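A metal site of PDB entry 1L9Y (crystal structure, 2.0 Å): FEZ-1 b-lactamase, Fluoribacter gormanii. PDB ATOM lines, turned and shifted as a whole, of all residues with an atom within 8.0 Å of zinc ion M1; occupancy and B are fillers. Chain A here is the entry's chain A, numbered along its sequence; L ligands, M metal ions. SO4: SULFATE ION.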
ATOM      1  N   TYR A   2      -9.520  11.006  -6.197  1.00  0.00           N
ATOM      2  CA  TYR A   2      -8.915  10.120  -7.188  1.00  0.00           C
ATOM      3  C   TYR A   2      -9.780  10.046  -8.437  1.00  0.00           C
ATOM      4  O   TYR A   2     -10.968   9.727  -8.356  1.00  0.00           O
ATOM      5  CB  TYR A   2      -8.721   8.705  -6.642  1.00  0.00           C
ATOM      6  CG  TYR A   2      -7.791   7.886  -7.504  1.00  0.00           C
ATOM      7  CD1 TYR A   2      -6.411   7.975  -7.349  1.00  0.00           C
ATOM      8  CD2 TYR A   2      -8.294   7.073  -8.527  1.00  0.00           C
ATOM      9  CE1 TYR A   2      -5.543   7.290  -8.188  1.00  0.00           C
ATOM     10  CE2 TYR A   2      -7.428   6.381  -9.377  1.00  0.00           C
ATOM     11  CZ  TYR A   2      -6.050   6.497  -9.196  1.00  0.00           C
ATOM     12  OH  TYR A   2      -5.176   5.843 -10.039  1.00  0.00           O
ATOM     13  N   ASP A  24      -7.119   2.495 -16.044  1.00  0.00           N
ATOM     14  CA  ASP A  24      -6.111   2.966 -15.096  1.00  0.00           C
ATOM     15  C   ASP A  24      -5.771   1.871 -14.087  1.00  0.00           C
ATOM     16  O   ASP A  24      -4.758   1.183 -14.217  1.00  0.00           O
ATOM     17  CB  ASP A  24      -6.616   4.202 -14.341  1.00  0.00           C
ATOM     18  CG  ASP A  24      -5.670   4.631 -13.224  1.00  0.00           C
ATOM     19  OD1 ASP A  24      -6.091   5.427 -12.355  1.00  0.00           O
ATOM     20  OD2 ASP A  24      -4.500   4.182 -13.217  1.00  0.00           O
ATOM     21  N   LEU A  25      -6.631   1.722 -13.074  1.00  0.00           N
ATOM     22  CA  LEU A  25      -6.430   0.700 -12.061  1.00  0.00           C
ATOM     23  C   LEU A  25      -6.489  -0.657 -12.769  1.00  0.00           C
ATOM     24  O   LEU A  25      -7.470  -0.981 -13.451  1.00  0.00           O
ATOM     25  CB  LEU A  25      -7.506   0.806 -10.980  1.00  0.00           C
ATOM     26  CG  LEU A  25      -7.593   2.194 -10.359  1.00  0.00           C
ATOM     27  CD1 LEU A  25      -8.666   2.215  -9.275  1.00  0.00           C
ATOM     28  CD2 LEU A  25      -6.217   2.595  -9.786  1.00  0.00           C
ATOM     29  N   ALA A  26      -5.424  -1.435 -12.625  1.00  0.00           N
ATOM     30  CA  ALA A  26      -5.354  -2.737 -13.287  1.00  0.00           C
ATOM     31  C   ALA A  26      -5.730  -3.907 -12.386  1.00  0.00           C
ATOM     32  O   ALA A  26      -5.296  -3.986 -11.228  1.00  0.00           O
ATOM     33  CB  ALA A  26      -3.944  -2.938 -13.835  1.00  0.00           C
ATOM     34  N   SER A  70      -2.046  -5.981  -5.151  1.00  0.00           N
ATOM     35  CA  SER A  70      -0.672  -5.564  -5.406  1.00  0.00           C
ATOM     36  C   SER A  70      -0.101  -4.945  -4.132  1.00  0.00           C
ATOM     37  O   SER A  70       1.018  -5.244  -3.730  1.00  0.00           O
ATOM     38  CB  SER A  70      -0.612  -4.551  -6.559  1.00  0.00           C
ATOM     39  OG  SER A  70      -0.997  -5.139  -7.786  1.00  0.00           O
ATOM     40  N   HIS A  71      -0.868  -4.060  -3.511  1.00  0.00           N
ATOM     41  CA  HIS A  71      -0.450  -3.423  -2.255  1.00  0.00           C
ATOM     42  C   HIS A  71      -1.636  -2.759  -1.567  1.00  0.00           C
ATOM     43  O   HIS A  71      -2.658  -2.463  -2.211  1.00  0.00           O
ATOM     44  CB  HIS A  71       0.693  -2.417  -2.468  1.00  0.00           C
ATOM     45  CG  HIS A  71       0.312  -1.194  -3.242  1.00  0.00           C
ATOM     46  ND1 HIS A  71       0.572  -1.048  -4.579  1.00  0.00           N
ATOM     47  CD2 HIS A  71      -0.279  -0.043  -2.839  1.00  0.00           C
ATOM     48  CE1 HIS A  71       0.161   0.135  -4.980  1.00  0.00           C
ATOM     49  NE2 HIS A  71      -0.368   0.774  -3.945  1.00  0.00           N
ATOM     50  N   HIS A  73      -3.473   0.002  -0.580  1.00  0.00           N
ATOM     51  CA  HIS A  73      -3.829   1.406  -0.791  1.00  0.00           C
ATOM     52  C   HIS A  73      -5.249   1.342  -1.379  1.00  0.00           C
ATOM     53  O   HIS A  73      -5.559   0.447  -2.165  1.00  0.00           O
ATOM     54  CB  HIS A  73      -2.852   2.095  -1.762  1.00  0.00           C
ATOM     55  CG  HIS A  73      -1.667   2.707  -1.080  1.00  0.00           C
ATOM     56  ND1 HIS A  73      -0.579   3.195  -1.764  1.00  0.00           N
ATOM     57  CD2 HIS A  73      -1.411   2.928   0.236  1.00  0.00           C
ATOM     58  CE1 HIS A  73       0.292   3.695  -0.904  1.00  0.00           C
ATOM     59  NE2 HIS A  73      -0.187   3.540   0.321  1.00  0.00           N
ATOM     60  N   PHE A  74      -6.111   2.274  -0.978  1.00  0.00           N
ATOM     61  CA  PHE A  74      -7.504   2.271  -1.431  1.00  0.00           C
ATOM     62  C   PHE A  74      -7.746   2.009  -2.921  1.00  0.00           C
ATOM     63  O   PHE A  74      -8.689   1.304  -3.269  1.00  0.00           O
ATOM     64  CB  PHE A  74      -8.183   3.589  -1.027  1.00  0.00           C
ATOM     65  CG  PHE A  74      -7.761   4.756  -1.870  1.00  0.00           C
ATOM     66  CD1 PHE A  74      -8.456   5.067  -3.043  1.00  0.00           C
ATOM     67  CD2 PHE A  74      -6.645   5.507  -1.532  1.00  0.00           C
ATOM     68  CE1 PHE A  74      -8.028   6.103  -3.864  1.00  0.00           C
ATOM     69  CE2 PHE A  74      -6.208   6.544  -2.364  1.00  0.00           C
ATOM     70  CZ  PHE A  74      -6.905   6.842  -3.529  1.00  0.00           C
ATOM     71  N   ASP A  75      -6.921   2.567  -3.800  1.00  0.00           N
ATOM     72  CA  ASP A  75      -7.154   2.363  -5.227  1.00  0.00           C
ATOM     73  C   ASP A  75      -6.939   0.930  -5.722  1.00  0.00           C
ATOM     74  O   ASP A  75      -7.280   0.605  -6.851  1.00  0.00           O
ATOM     75  CB  ASP A  75      -6.321   3.331  -6.066  1.00  0.00           C
ATOM     76  CG  ASP A  75      -4.839   3.183  -5.837  1.00  0.00           C
ATOM     77  OD1 ASP A  75      -4.076   3.514  -6.762  1.00  0.00           O
ATOM     78  OD2 ASP A  75      -4.423   2.753  -4.736  1.00  0.00           O
ATOM     79  N   HIS A  76      -6.380   0.079  -4.866  1.00  0.00           N
ATOM     80  CA  HIS A  76      -6.146  -1.307  -5.259  1.00  0.00           C
ATOM     81  C   HIS A  76      -6.898  -2.300  -4.389  1.00  0.00           C
ATOM     82  O   HIS A  76      -7.178  -3.421  -4.827  1.00  0.00           O
ATOM     83  CB  HIS A  76      -4.648  -1.628  -5.223  1.00  0.00           C
ATOM     84  CG  HIS A  76      -3.842  -0.757  -6.123  1.00  0.00           C
ATOM     85  ND1 HIS A  76      -4.004  -0.750  -7.487  1.00  0.00           N
ATOM     86  CD2 HIS A  76      -2.933   0.212  -5.849  1.00  0.00           C
ATOM     87  CE1 HIS A  76      -3.237   0.190  -8.021  1.00  0.00           C
ATOM     88  NE2 HIS A  76      -2.579   0.788  -7.044  1.00  0.00           N
ATOM     89  N   HIS A 149       6.769   1.309  -1.186  1.00  0.00           N
ATOM     90  CA  HIS A 149       5.531   2.002  -1.534  1.00  0.00           C
ATOM     91  C   HIS A 149       4.521   1.758  -0.401  1.00  0.00           C
ATOM     92  O   HIS A 149       3.771   2.646  -0.016  1.00  0.00           O
ATOM     93  CB  HIS A 149       4.985   1.471  -2.852  1.00  0.00           C
ATOM     94  CG  HIS A 149       3.877   2.289  -3.395  1.00  0.00           C
ATOM     95  ND1 HIS A 149       4.073   3.549  -3.927  1.00  0.00           N
ATOM     96  CD2 HIS A 149       2.541   2.062  -3.439  1.00  0.00           C
ATOM     97  CE1 HIS A 149       2.913   4.065  -4.268  1.00  0.00           C
ATOM     98  NE2 HIS A 149       1.969   3.187  -3.987  1.00  0.00           N
ATOM     99  N   GLY A 173       4.073  -4.539  -8.226  1.00  0.00           N
ATOM    100  CA  GLY A 173       3.208  -3.920  -7.227  1.00  0.00           C
ATOM    101  C   GLY A 173       3.246  -2.414  -7.213  1.00  0.00           C
ATOM    102  O   GLY A 173       2.205  -1.764  -7.070  1.00  0.00           O
ATOM    103  N   SER A 174       4.464  -1.868  -7.358  1.00  0.00           N
ATOM    104  CA  SER A 174       4.761  -0.435  -7.376  1.00  0.00           C
ATOM    105  C   SER A 174       5.943  -0.087  -6.485  1.00  0.00           C
ATOM    106  O   SER A 174       5.996  -0.506  -5.340  1.00  0.00           O
ATOM    107  CB  SER A 174       3.569   0.413  -6.913  1.00  0.00           C
ATOM    108  OG  SER A 174       3.946   1.786  -6.835  1.00  0.00           O
ATOM    109  N   ASN A 178       5.296   8.143  -3.359  1.00  0.00           N
ATOM    110  CA  ASN A 178       4.153   9.051  -3.337  1.00  0.00           C
ATOM    111  C   ASN A 178       4.537  10.417  -2.779  1.00  0.00           C
ATOM    112  O   ASN A 178       5.317  10.533  -1.835  1.00  0.00           O
ATOM    113  CB  ASN A 178       3.014   8.490  -2.502  1.00  0.00           C
ATOM    114  CG  ASN A 178       2.153   7.495  -3.257  1.00  0.00           C
ATOM    115  OD1 ASN A 178       2.278   7.334  -4.480  1.00  0.00           O
ATOM    116  ND2 ASN A 178       1.265   6.818  -2.545  1.00  0.00           N
ATOM    117  N   SER A 214       0.233  -2.666 -11.361  1.00  0.00           N
ATOM    118  CA  SER A 214      -0.996  -2.308 -10.666  1.00  0.00           C
ATOM    119  C   SER A 214      -1.732  -1.192 -11.391  1.00  0.00           C
ATOM    120  O   SER A 214      -2.937  -1.007 -11.198  1.00  0.00           O
ATOM    121  CB  SER A 214      -0.691  -1.915  -9.222  1.00  0.00           C
ATOM    122  OG  SER A 214       0.391  -0.994  -9.163  1.00  0.00           O
ATOM    123  N   HIS A 215      -1.006  -0.443 -12.222  1.00  0.00           N
ATOM    124  CA  HIS A 215      -1.596   0.660 -12.989  1.00  0.00           C
ATOM    125  C   HIS A 215      -1.332   0.460 -14.485  1.00  0.00           C
ATOM    126  O   HIS A 215      -0.211   0.128 -14.881  1.00  0.00           O
ATOM    127  CB  HIS A 215      -1.006   1.995 -12.563  1.00  0.00           C
ATOM    128  CG  HIS A 215      -1.564   2.515 -11.276  1.00  0.00           C
ATOM    129  ND1 HIS A 215      -2.712   3.277 -11.204  1.00  0.00           N
ATOM    130  CD2 HIS A 215      -1.130   2.379  -9.998  1.00  0.00           C
ATOM    131  CE1 HIS A 215      -2.958   3.586  -9.951  1.00  0.00           C
ATOM    132  NE2 HIS A 215      -2.014   3.053  -9.191  1.00  0.00           N
ATOM    133  N   MET A 218       1.675   2.053 -16.205  1.00  0.00           N
ATOM    134  CA  MET A 218       2.996   1.502 -15.923  1.00  0.00           C
ATOM    135  C   MET A 218       3.541   0.721 -17.103  1.00  0.00           C
ATOM    136  O   MET A 218       4.731   0.829 -17.425  1.00  0.00           O
ATOM    137  CB  MET A 218       2.949   0.569 -14.711  1.00  0.00           C
ATOM    138  CG  MET A 218       2.585   1.216 -13.397  1.00  0.00           C
ATOM    139  SD  MET A 218       2.510  -0.006 -12.074  1.00  0.00           S
ATOM    140  CE  MET A 218       2.563   1.037 -10.604  1.00  0.00           C
HETATM  141  S   SO4 L   1      -1.147   5.914  -5.539  1.00  0.00           S
HETATM  142  O1  SO4 L   1      -2.460   6.439  -5.100  1.00  0.00           O
HETATM  143  O2  SO4 L   1      -0.306   7.033  -6.007  1.00  0.00           O
HETATM  144  O3  SO4 L   1      -1.354   4.988  -6.646  1.00  0.00           O
HETATM  145  O4  SO4 L   1      -0.479   5.253  -4.412  1.00  0.00           O
HETATM  146 ZN    ZN M   1      -1.966   2.886  -7.035  1.00  0.00          ZN
HETATM  147 ZN    ZN M   2      -0.161   3.019  -3.890  1.00  0.00          ZN
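ND1 of His 215 is in hydrogen-bond range of OD2 of Asp 24, 2.8 Å away.
The backbone NH (N) of His 215 is in hydrogen-bond range of the side-chain sulfur (SD) of Met 218 (3.5 Å).
Three residues have an atom within 4 Å of zinc ion M1: Asp 75, His 76 and His 215.
The nearest printed residue that does not touch zinc ion M1 is His 71 (4.04 Å).
A ring nitrogen (NE2) of His 215 binds zinc ion M1, 2.2 Å away.
NE2 of His 76 binds zinc ion M1, 2.2 Å away.
OD1 of Asp 75 is bound to zinc ion M1, at 2.2 Å.
Zinc ion M1 is bound by O3 of the ligand (2.2 Å).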
